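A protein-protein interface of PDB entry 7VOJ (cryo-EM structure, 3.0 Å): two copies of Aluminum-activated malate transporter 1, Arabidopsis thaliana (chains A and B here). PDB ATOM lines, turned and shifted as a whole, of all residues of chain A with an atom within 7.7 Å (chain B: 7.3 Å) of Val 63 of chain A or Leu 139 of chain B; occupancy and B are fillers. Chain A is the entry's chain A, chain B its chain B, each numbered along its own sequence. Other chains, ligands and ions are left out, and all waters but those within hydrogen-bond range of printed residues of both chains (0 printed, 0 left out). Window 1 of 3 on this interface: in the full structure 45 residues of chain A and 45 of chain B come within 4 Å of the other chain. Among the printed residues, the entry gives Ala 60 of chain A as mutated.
Hydrophobic or aromatic side chains of chain B within 4 Å of the printed part of chain A: Val 114, Ala 118, Leu 139, Ile 142, Leu 143 and Ala 146. Of the 18 printed residues of chain A, 4 touch a printed residue of chain B. Hydrophobic or aromatic side chains of chain A within 4 Å of the printed part of chain B: Leu 32, Val 59, Ala 60 and Val 63. Among the printed residues, 6 pairs touch across the chains. Among the printed residues, no Asp or Glu carboxylate lies within 4 Å of a Lys or Arg side-chain nitrogen of the other chain.
Of chain B, only Leu 139 (3.7 Å) and Ile 142 (3.8 Å) come within 4 Å of Val 63 of chain A. Leu 139 of chain B touches one residue of chain A. Of the printed residues of chain A, Val 114 of chain B touches Leu 32. Of the printed residues of chain A, Ile 142 of chain B touches Val 63. Printed residues of chain B within 4 Å of Leu 32 of chain A: Val 114 and Ala 118. Printed residues of chain B within 4 Å of Val 59 of chain A: Ala 146 (3.8 Å). The nearest residue of chain B that does not touch Val 63 of chain A is Leu 143 of chain B (4.2 Å). The nearest residue of chain A that does not touch Leu 139 of chain B is Val 64 of chain A (4.5 Å). The nearest printed residue of chain A that does not touch Ala 118 of chain B is Val 28 of chain A (4.4 Å).
No position is printed for both chains. Of the 6 pairs that touch across the chains among the printed residues, none has its exchanged pair printed and touching as well.
Among the printed residues, pairs that only touch across the chains: Val 63 of chain A with Leu 139 of chain B (3.7 Å), Ala 60 of chain A with Leu 143 of chain B (3.7 Å), Leu 32 of chain A with Ala 118 of chain B (3.8 Å), Val 59 of chain A with Ala 146 of chain B (3.8 Å), Val 63 of chain A with Ile 142 of chain B (3.8 Å) and Leu 32 of chain A with Val 114 of chain B (3.9 Å).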
ATOM      1  N   VAL A  28       9.690 -31.696  18.271  1.00  0.00           N
ATOM      2  CA  VAL A  28       9.784 -31.062  16.956  1.00  0.00           C
ATOM      3  C   VAL A  28      10.786 -31.791  16.069  1.00  0.00           C
ATOM      4  O   VAL A  28      10.495 -32.096  14.905  1.00  0.00           O
ATOM      5  CB  VAL A  28      10.123 -29.572  17.112  1.00  0.00           C
ATOM      6  CG1 VAL A  28      10.665 -28.995  15.831  1.00  0.00           C
ATOM      7  CG2 VAL A  28       8.882 -28.836  17.500  1.00  0.00           C
ATOM      8  N   ALA A  31       9.340 -35.045  14.826  1.00  0.00           N
ATOM      9  CA  ALA A  31       8.403 -34.913  13.712  1.00  0.00           C
ATOM     10  C   ALA A  31       9.127 -34.667  12.396  1.00  0.00           C
ATOM     11  O   ALA A  31       8.696 -35.166  11.349  1.00  0.00           O
ATOM     12  CB  ALA A  31       7.404 -33.800  13.989  1.00  0.00           C
ATOM     13  N   LEU A  32      10.241 -33.929  12.434  1.00  0.00           N
ATOM     14  CA  LEU A  32      11.036 -33.720  11.224  1.00  0.00           C
ATOM     15  C   LEU A  32      11.661 -35.015  10.730  1.00  0.00           C
ATOM     16  O   LEU A  32      11.638 -35.294   9.527  1.00  0.00           O
ATOM     17  CB  LEU A  32      12.126 -32.686  11.467  1.00  0.00           C
ATOM     18  CG  LEU A  32      11.698 -31.229  11.508  1.00  0.00           C
ATOM     19  CD1 LEU A  32      12.897 -30.353  11.451  1.00  0.00           C
ATOM     20  CD2 LEU A  32      10.831 -30.935  10.343  1.00  0.00           C
ATOM     21  N   TRP A  57       7.959 -29.467   0.888  1.00  0.00           N
ATOM     22  CA  TRP A  57       6.765 -28.831   1.418  1.00  0.00           C
ATOM     23  C   TRP A  57       6.235 -29.518   2.667  1.00  0.00           C
ATOM     24  O   TRP A  57       5.626 -28.848   3.506  1.00  0.00           O
ATOM     25  CB  TRP A  57       5.680 -28.814   0.358  1.00  0.00           C
ATOM     26  CG  TRP A  57       5.889 -27.859  -0.742  1.00  0.00           C
ATOM     27  CD1 TRP A  57       6.796 -26.859  -0.792  1.00  0.00           C
ATOM     28  CD2 TRP A  57       5.159 -27.803  -1.963  1.00  0.00           C
ATOM     29  NE1 TRP A  57       6.682 -26.177  -1.972  1.00  0.00           N
ATOM     30  CE2 TRP A  57       5.679 -26.745  -2.710  1.00  0.00           C
ATOM     31  CE3 TRP A  57       4.116 -28.553  -2.499  1.00  0.00           C
ATOM     32  CZ2 TRP A  57       5.192 -26.413  -3.957  1.00  0.00           C
ATOM     33  CZ3 TRP A  57       3.638 -28.224  -3.735  1.00  0.00           C
ATOM     34  CH2 TRP A  57       4.172 -27.163  -4.451  1.00  0.00           C
ATOM     35  N   ALA A  58       6.450 -30.826   2.815  1.00  0.00           N
ATOM     36  CA  ALA A  58       6.064 -31.503   4.046  1.00  0.00           C
ATOM     37  C   ALA A  58       6.900 -31.024   5.217  1.00  0.00           C
ATOM     38  O   ALA A  58       6.387 -30.846   6.322  1.00  0.00           O
ATOM     39  CB  ALA A  58       6.208 -33.008   3.888  1.00  0.00           C
ATOM     40  N   VAL A  59       8.184 -30.779   4.983  1.00  0.00           N
ATOM     41  CA  VAL A  59       9.056 -30.290   6.038  1.00  0.00           C
ATOM     42  C   VAL A  59       8.778 -28.823   6.337  1.00  0.00           C
ATOM     43  O   VAL A  59       8.883 -28.396   7.493  1.00  0.00           O
ATOM     44  CB  VAL A  59      10.512 -30.553   5.632  1.00  0.00           C
ATOM     45  CG1 VAL A  59      11.427 -30.207   6.728  1.00  0.00           C
ATOM     46  CG2 VAL A  59      10.686 -32.007   5.303  1.00  0.00           C
ATOM     47  N   ALA A  60       8.389 -28.037   5.324  1.00  0.00           N
ATOM     48  CA  ALA A  60       7.907 -26.678   5.572  1.00  0.00           C
ATOM     49  C   ALA A  60       6.677 -26.687   6.462  1.00  0.00           C
ATOM     50  O   ALA A  60       6.572 -25.883   7.393  1.00  0.00           O
ATOM     51  CB  ALA A  60       7.608 -25.974   4.258  1.00  0.00           C
ATOM     52  N   THR A  61       5.751 -27.608   6.200  1.00  0.00           N
ATOM     53  CA  THR A  61       4.534 -27.706   6.994  1.00  0.00           C
ATOM     54  C   THR A  61       4.835 -28.089   8.431  1.00  0.00           C
ATOM     55  O   THR A  61       4.302 -27.478   9.354  1.00  0.00           O
ATOM     56  CB  THR A  61       3.594 -28.716   6.361  1.00  0.00           C
ATOM     57  OG1 THR A  61       3.242 -28.267   5.052  1.00  0.00           O
ATOM     58  CG2 THR A  61       2.341 -28.878   7.176  1.00  0.00           C
ATOM     59  N   VAL A  62       5.723 -29.059   8.641  1.00  0.00           N
ATOM     60  CA  VAL A  62       6.012 -29.527   9.994  1.00  0.00           C
ATOM     61  C   VAL A  62       6.736 -28.464  10.809  1.00  0.00           C
ATOM     62  O   VAL A  62       6.448 -28.287  11.996  1.00  0.00           O
ATOM     63  CB  VAL A  62       6.795 -30.849   9.926  1.00  0.00           C
ATOM     64  CG1 VAL A  62       7.281 -31.266  11.270  1.00  0.00           C
ATOM     65  CG2 VAL A  62       5.905 -31.928   9.393  1.00  0.00           C
ATOM     66  N   VAL A  63       7.632 -27.699  10.186  1.00  0.00           N
ATOM     67  CA  VAL A  63       8.334 -26.647  10.914  1.00  0.00           C
ATOM     68  C   VAL A  63       7.379 -25.524  11.296  1.00  0.00           C
ATOM     69  O   VAL A  63       7.412 -25.029  12.427  1.00  0.00           O
ATOM     70  CB  VAL A  63       9.521 -26.138  10.080  1.00  0.00           C
ATOM     71  CG1 VAL A  63      10.075 -24.858  10.634  1.00  0.00           C
ATOM     72  CG2 VAL A  63      10.597 -27.178  10.045  1.00  0.00           C
ATOM     73  N   VAL A  64       6.470 -25.154  10.397  1.00  0.00           N
ATOM     74  CA  VAL A  64       5.601 -24.012  10.663  1.00  0.00           C
ATOM     75  C   VAL A  64       4.475 -24.377  11.630  1.00  0.00           C
ATOM     76  O   VAL A  64       4.186 -23.626  12.565  1.00  0.00           O
ATOM     77  CB  VAL A  64       5.070 -23.447   9.337  1.00  0.00           C
ATOM     78  CG1 VAL A  64       4.066 -22.395   9.589  1.00  0.00           C
ATOM     79  CG2 VAL A  64       6.206 -22.849   8.552  1.00  0.00           C
ATOM     80  N   VAL A  65       3.821 -25.499  11.353  1.00  0.00           N
ATOM     81  CA  VAL A  65       2.688 -25.982  12.133  1.00  0.00           C
ATOM     82  C   VAL A  65       2.946 -26.354  13.589  1.00  0.00           C
ATOM     83  O   VAL A  65       2.120 -26.063  14.448  1.00  0.00           O
ATOM     84  CB  VAL A  65       2.019 -27.184  11.445  1.00  0.00           C
ATOM     85  CG1 VAL A  65       1.061 -27.872  12.402  1.00  0.00           C
ATOM     86  CG2 VAL A  65       1.300 -26.737  10.184  1.00  0.00           C
ATOM     87  N   PHE A  66       4.073 -26.992  13.879  1.00  0.00           N
ATOM     88  CA  PHE A  66       4.328 -27.412  15.252  1.00  0.00           C
ATOM     89  C   PHE A  66       4.416 -26.226  16.204  1.00  0.00           C
ATOM     90  O   PHE A  66       5.103 -25.244  15.935  1.00  0.00           O
ATOM     91  CB  PHE A  66       5.595 -28.261  15.334  1.00  0.00           C
ATOM     92  CG  PHE A  66       5.483 -29.414  16.287  1.00  0.00           C
ATOM     93  CD1 PHE A  66       5.715 -29.240  17.637  1.00  0.00           C
ATOM     94  CD2 PHE A  66       5.133 -30.672  15.831  1.00  0.00           C
ATOM     95  CE1 PHE A  66       5.606 -30.299  18.515  1.00  0.00           C
ATOM     96  CE2 PHE A  66       5.022 -31.735  16.702  1.00  0.00           C
ATOM     97  CZ  PHE A  66       5.260 -31.549  18.047  1.00  0.00           C
ATOM     98  N   GLU A  67       3.726 -26.349  17.334  1.00  0.00           N
ATOM     99  CA  GLU A  67       3.672 -25.310  18.360  1.00  0.00           C
ATOM    100  C   GLU A  67       3.688 -25.929  19.753  1.00  0.00           C
ATOM    101  O   GLU A  67       3.450 -27.124  19.907  1.00  0.00           O
ATOM    102  CB  GLU A  67       2.462 -24.392  18.170  1.00  0.00           C
ATOM    103  CG  GLU A  67       2.579 -23.473  16.965  1.00  0.00           C
ATOM    104  CD  GLU A  67       1.876 -22.148  17.166  1.00  0.00           C
ATOM    105  OE1 GLU A  67       1.668 -21.757  18.333  1.00  0.00           O
ATOM    106  OE2 GLU A  67       1.538 -21.495  16.158  1.00  0.00           O
ATOM    107  N   LYS A  76      -3.199 -24.214  13.834  1.00  0.00           N
ATOM    108  CA  LYS A  76      -2.385 -23.976  12.648  1.00  0.00           C
ATOM    109  C   LYS A  76      -2.554 -25.070  11.612  1.00  0.00           C
ATOM    110  O   LYS A  76      -2.599 -24.780  10.417  1.00  0.00           O
ATOM    111  CB  LYS A  76      -0.919 -23.849  13.020  1.00  0.00           C
ATOM    112  CG  LYS A  76      -0.540 -22.491  13.500  1.00  0.00           C
ATOM    113  CD  LYS A  76       0.882 -22.185  13.154  1.00  0.00           C
ATOM    114  CE  LYS A  76       1.177 -20.721  13.335  1.00  0.00           C
ATOM    115  NZ  LYS A  76       2.567 -20.379  12.938  1.00  0.00           N
ATOM    116  N   ARG A  80      -4.250 -24.364   7.920  1.00  0.00           N
ATOM    117  CA  ARG A  80      -3.463 -24.663   6.732  1.00  0.00           C
ATOM    118  C   ARG A  80      -4.124 -25.713   5.856  1.00  0.00           C
ATOM    119  O   ARG A  80      -4.071 -25.605   4.631  1.00  0.00           O
ATOM    120  CB  ARG A  80      -2.078 -25.124   7.144  1.00  0.00           C
ATOM    121  CG  ARG A  80      -1.059 -25.063   6.069  1.00  0.00           C
ATOM    122  CD  ARG A  80       0.292 -25.416   6.612  1.00  0.00           C
ATOM    123  NE  ARG A  80       1.299 -25.417   5.566  1.00  0.00           N
ATOM    124  CZ  ARG A  80       2.205 -24.468   5.411  1.00  0.00           C
ATOM    125  NH1 ARG A  80       2.234 -23.447   6.241  1.00  0.00           N
ATOM    126  NH2 ARG A  80       3.086 -24.540   4.432  1.00  0.00           N
ATOM    127  N   GLY A 172       2.064 -33.638   6.474  1.00  0.00           N
ATOM    128  CA  GLY A 172       2.846 -32.901   7.459  1.00  0.00           C
ATOM    129  C   GLY A 172       2.036 -32.475   8.671  1.00  0.00           C
ATOM    130  O   GLY A 172       2.507 -32.571   9.809  1.00  0.00           O
ATOM    131  N   CYS A 176       2.387 -33.848  12.654  1.00  0.00           N
ATOM    132  CA  CYS A 176       2.525 -32.900  13.757  1.00  0.00           C
ATOM    133  C   CYS A 176       1.495 -33.137  14.848  1.00  0.00           C
ATOM    134  O   CYS A 176       1.840 -33.159  16.027  1.00  0.00           O
ATOM    135  CB  CYS A 176       2.384 -31.477  13.246  1.00  0.00           C
ATOM    136  SG  CYS A 176       3.890 -30.761  12.684  1.00  0.00           S
ATOM    137  N   ALA B  83      18.218 -14.829   8.384  1.00  0.00           N
ATOM    138  CA  ALA B  83      18.064 -16.249   8.674  1.00  0.00           C
ATOM    139  C   ALA B  83      18.351 -17.108   7.454  1.00  0.00           C
ATOM    140  O   ALA B  83      18.987 -18.160   7.573  1.00  0.00           O
ATOM    141  CB  ALA B  83      16.664 -16.536   9.189  1.00  0.00           C
ATOM    142  N   VAL B 114      19.822 -32.421  11.040  1.00  0.00           N
ATOM    143  CA  VAL B 114      18.583 -31.646  11.032  1.00  0.00           C
ATOM    144  C   VAL B 114      17.849 -31.795  12.358  1.00  0.00           C
ATOM    145  O   VAL B 114      17.310 -30.816  12.885  1.00  0.00           O
ATOM    146  CB  VAL B 114      17.712 -32.042   9.828  1.00  0.00           C
ATOM    147  CG1 VAL B 114      16.317 -31.484   9.931  1.00  0.00           C
ATOM    148  CG2 VAL B 114      18.344 -31.521   8.569  1.00  0.00           C
ATOM    149  N   ALA B 118      17.151 -28.463  14.824  1.00  0.00           N
ATOM    150  CA  ALA B 118      15.760 -28.158  15.117  1.00  0.00           C
ATOM    151  C   ALA B 118      15.533 -28.148  16.618  1.00  0.00           C
ATOM    152  O   ALA B 118      14.846 -27.276  17.143  1.00  0.00           O
ATOM    153  CB  ALA B 118      14.843 -29.166  14.445  1.00  0.00           C
ATOM    154  N   SER B 121      17.247 -24.961  18.106  1.00  0.00           N
ATOM    155  CA  SER B 121      16.564 -23.719  17.776  1.00  0.00           C
ATOM    156  C   SER B 121      15.158 -23.652  18.358  1.00  0.00           C
ATOM    157  O   SER B 121      14.708 -22.566  18.741  1.00  0.00           O
ATOM    158  CB  SER B 121      16.531 -23.538  16.272  1.00  0.00           C
ATOM    159  OG  SER B 121      17.837 -23.370  15.777  1.00  0.00           O
ATOM    160  N   ARG B 125      13.792 -20.669  20.998  1.00  0.00           N
ATOM    161  CA  ARG B 125      12.585 -19.859  20.813  1.00  0.00           C
ATOM    162  C   ARG B 125      11.766 -19.632  22.085  1.00  0.00           C
ATOM    163  O   ARG B 125      10.713 -18.998  21.995  1.00  0.00           O
ATOM    164  CB  ARG B 125      11.676 -20.497  19.773  1.00  0.00           C
ATOM    165  CG  ARG B 125      12.148 -20.328  18.368  1.00  0.00           C
ATOM    166  CD  ARG B 125      11.203 -20.977  17.415  1.00  0.00           C
ATOM    167  NE  ARG B 125       9.985 -20.205  17.293  1.00  0.00           N
ATOM    168  CZ  ARG B 125       8.906 -20.630  16.658  1.00  0.00           C
ATOM    169  NH1 ARG B 125       8.900 -21.826  16.098  1.00  0.00           N
ATOM    170  NH2 ARG B 125       7.831 -19.865  16.591  1.00  0.00           N
ATOM    171  N   PHE B 134      13.205 -11.609  17.786  1.00  0.00           N
ATOM    172  CA  PHE B 134      13.570 -12.380  16.604  1.00  0.00           C
ATOM    173  C   PHE B 134      13.028 -13.799  16.590  1.00  0.00           C
ATOM    174  O   PHE B 134      13.784 -14.729  16.320  1.00  0.00           O
ATOM    175  CB  PHE B 134      15.084 -12.490  16.468  1.00  0.00           C
ATOM    176  CG  PHE B 134      15.835 -11.290  16.918  1.00  0.00           C
ATOM    177  CD1 PHE B 134      15.976 -10.198  16.093  1.00  0.00           C
ATOM    178  CD2 PHE B 134      16.448 -11.273  18.146  1.00  0.00           C
ATOM    179  CE1 PHE B 134      16.687  -9.102  16.501  1.00  0.00           C
ATOM    180  CE2 PHE B 134      17.156 -10.179  18.558  1.00  0.00           C
ATOM    181  CZ  PHE B 134      17.277  -9.095  17.733  1.00  0.00           C
ATOM    182  N   ASP B 135      11.752 -14.003  16.886  1.00  0.00           N
ATOM    183  CA  ASP B 135      11.223 -15.360  16.867  1.00  0.00           C
ATOM    184  C   ASP B 135      11.064 -15.883  15.446  1.00  0.00           C
ATOM    185  O   ASP B 135      11.326 -17.062  15.173  1.00  0.00           O
ATOM    186  CB  ASP B 135       9.889 -15.405  17.601  1.00  0.00           C
ATOM    187  CG  ASP B 135       9.112 -16.664  17.312  1.00  0.00           C
ATOM    188  OD1 ASP B 135       9.521 -17.737  17.792  1.00  0.00           O
ATOM    189  OD2 ASP B 135       8.096 -16.589  16.595  1.00  0.00           O
ATOM    190  N   TYR B 136      10.664 -15.012  14.526  1.00  0.00           N
ATOM    191  CA  TYR B 136      10.481 -15.406  13.138  1.00  0.00           C
ATOM    192  C   TYR B 136      11.809 -15.698  12.460  1.00  0.00           C
ATOM    193  O   TYR B 136      11.868 -16.508  11.532  1.00  0.00           O
ATOM    194  CB  TYR B 136       9.725 -14.303  12.410  1.00  0.00           C
ATOM    195  CG  TYR B 136       9.431 -14.585  10.973  1.00  0.00           C
ATOM    196  CD1 TYR B 136       8.452 -15.490  10.616  1.00  0.00           C
ATOM    197  CD2 TYR B 136      10.119 -13.926   9.973  1.00  0.00           C
ATOM    198  CE1 TYR B 136       8.181 -15.739   9.306  1.00  0.00           C
ATOM    199  CE2 TYR B 136       9.854 -14.171   8.669  1.00  0.00           C
ATOM    200  CZ  TYR B 136       8.886 -15.074   8.343  1.00  0.00           C
ATOM    201  OH  TYR B 136       8.632 -15.316   7.030  1.00  0.00           O
ATOM    202  N   GLY B 137      12.885 -15.071  12.921  1.00  0.00           N
ATOM    203  CA  GLY B 137      14.196 -15.404  12.404  1.00  0.00           C
ATOM    204  C   GLY B 137      14.637 -16.799  12.788  1.00  0.00           C
ATOM    205  O   GLY B 137      15.293 -17.484  12.008  1.00  0.00           O
ATOM    206  N   ILE B 138      14.262 -17.255  13.981  1.00  0.00           N
ATOM    207  CA  ILE B 138      14.635 -18.609  14.364  1.00  0.00           C
ATOM    208  C   ILE B 138      13.767 -19.622  13.635  1.00  0.00           C
ATOM    209  O   ILE B 138      14.233 -20.716  13.297  1.00  0.00           O
ATOM    210  CB  ILE B 138      14.564 -18.777  15.889  1.00  0.00           C
ATOM    211  CG1 ILE B 138      15.320 -17.655  16.580  1.00  0.00           C
ATOM    212  CG2 ILE B 138      15.203 -20.059  16.313  1.00  0.00           C
ATOM    213  CD1 ILE B 138      16.787 -17.608  16.266  1.00  0.00           C
ATOM    214  N   LEU B 139      12.519 -19.268  13.331  1.00  0.00           N
ATOM    215  CA  LEU B 139      11.687 -20.162  12.533  1.00  0.00           C
ATOM    216  C   LEU B 139      12.224 -20.325  11.115  1.00  0.00           C
ATOM    217  O   LEU B 139      12.301 -21.443  10.602  1.00  0.00           O
ATOM    218  CB  LEU B 139      10.261 -19.642  12.494  1.00  0.00           C
ATOM    219  CG  LEU B 139       9.300 -20.543  11.748  1.00  0.00           C
ATOM    220  CD1 LEU B 139       8.958 -21.693  12.631  1.00  0.00           C
ATOM    221  CD2 LEU B 139       8.067 -19.783  11.356  1.00  0.00           C
ATOM    222  N   ILE B 140      12.636 -19.228  10.479  1.00  0.00           N
ATOM    223  CA  ILE B 140      13.200 -19.315   9.135  1.00  0.00           C
ATOM    224  C   ILE B 140      14.582 -19.963   9.167  1.00  0.00           C
ATOM    225  O   ILE B 140      15.008 -20.579   8.185  1.00  0.00           O
ATOM    226  CB  ILE B 140      13.197 -17.911   8.499  1.00  0.00           C
ATOM    227  CG1 ILE B 140      11.768 -17.421   8.384  1.00  0.00           C
ATOM    228  CG2 ILE B 140      13.769 -17.884   7.106  1.00  0.00           C
ATOM    229  CD1 ILE B 140      10.894 -18.309   7.570  1.00  0.00           C
ATOM    230  N   PHE B 141      15.273 -19.903  10.306  1.00  0.00           N
ATOM    231  CA  PHE B 141      16.536 -20.617  10.448  1.00  0.00           C
ATOM    232  C   PHE B 141      16.327 -22.124  10.386  1.00  0.00           C
ATOM    233  O   PHE B 141      17.027 -22.823   9.641  1.00  0.00           O
ATOM    234  CB  PHE B 141      17.198 -20.214  11.757  1.00  0.00           C
ATOM    235  CG  PHE B 141      18.595 -20.694  11.901  1.00  0.00           C
ATOM    236  CD1 PHE B 141      19.584 -20.210  11.083  1.00  0.00           C
ATOM    237  CD2 PHE B 141      18.927 -21.622  12.860  1.00  0.00           C
ATOM    238  CE1 PHE B 141      20.877 -20.648  11.216  1.00  0.00           C
ATOM    239  CE2 PHE B 141      20.219 -22.052  12.996  1.00  0.00           C
ATOM    240  CZ  PHE B 141      21.192 -21.570  12.171  1.00  0.00           C
ATOM    241  N   ILE B 142      15.338 -22.631  11.134  1.00  0.00           N
ATOM    242  CA  ILE B 142      14.978 -24.051  11.081  1.00  0.00           C
ATOM    243  C   ILE B 142      14.546 -24.448   9.680  1.00  0.00           C
ATOM    244  O   ILE B 142      14.959 -25.489   9.155  1.00  0.00           O
ATOM    245  CB  ILE B 142      13.857 -24.367  12.085  1.00  0.00           C
ATOM    246  CG1 ILE B 142      14.226 -23.965  13.491  1.00  0.00           C
ATOM    247  CG2 ILE B 142      13.554 -25.830  12.092  1.00  0.00           C
ATOM    248  CD1 ILE B 142      13.063 -24.058  14.426  1.00  0.00           C
ATOM    249  N   LEU B 143      13.736 -23.602   9.046  1.00  0.00           N
ATOM    250  CA  LEU B 143      13.148 -23.917   7.752  1.00  0.00           C
ATOM    251  C   LEU B 143      14.198 -23.991   6.658  1.00  0.00           C
ATOM    252  O   LEU B 143      14.202 -24.932   5.864  1.00  0.00           O
ATOM    253  CB  LEU B 143      12.112 -22.861   7.402  1.00  0.00           C
ATOM    254  CG  LEU B 143      11.407 -22.931   6.067  1.00  0.00           C
ATOM    255  CD1 LEU B 143      10.618 -24.202   6.024  1.00  0.00           C
ATOM    256  CD2 LEU B 143      10.509 -21.765   5.947  1.00  0.00           C
ATOM    257  N   THR B 144      15.092 -23.014   6.599  1.00  0.00           N
ATOM    258  CA  THR B 144      16.062 -22.972   5.518  1.00  0.00           C
ATOM    259  C   THR B 144      17.126 -24.046   5.672  1.00  0.00           C
ATOM    260  O   THR B 144      17.566 -24.626   4.670  1.00  0.00           O
ATOM    261  CB  THR B 144      16.686 -21.595   5.458  1.00  0.00           C
ATOM    262  OG1 THR B 144      15.641 -20.628   5.463  1.00  0.00           O
ATOM    263  CG2 THR B 144      17.473 -21.433   4.209  1.00  0.00           C
ATOM    264  N   PHE B 145      17.524 -24.356   6.912  1.00  0.00           N
ATOM    265  CA  PHE B 145      18.463 -25.455   7.110  1.00  0.00           C
ATOM    266  C   PHE B 145      17.844 -26.776   6.701  1.00  0.00           C
ATOM    267  O   PHE B 145      18.505 -27.610   6.073  1.00  0.00           O
ATOM    268  CB  PHE B 145      18.914 -25.516   8.563  1.00  0.00           C
ATOM    269  CG  PHE B 145      20.083 -26.418   8.799  1.00  0.00           C
ATOM    270  CD1 PHE B 145      21.366 -25.932   8.711  1.00  0.00           C
ATOM    271  CD2 PHE B 145      19.905 -27.746   9.128  1.00  0.00           C
ATOM    272  CE1 PHE B 145      22.444 -26.754   8.936  1.00  0.00           C
ATOM    273  CE2 PHE B 145      20.975 -28.568   9.354  1.00  0.00           C
ATOM    274  CZ  PHE B 145      22.244 -28.074   9.256  1.00  0.00           C
ATOM    275  N   ALA B 146      16.575 -26.980   7.017  1.00  0.00           N
ATOM    276  CA  ALA B 146      15.954 -28.240   6.661  1.00  0.00           C
ATOM    277  C   ALA B 146      15.592 -28.331   5.183  1.00  0.00           C
ATOM    278  O   ALA B 146      15.438 -29.439   4.672  1.00  0.00           O
ATOM    279  CB  ALA B 146      14.725 -28.461   7.532  1.00  0.00           C
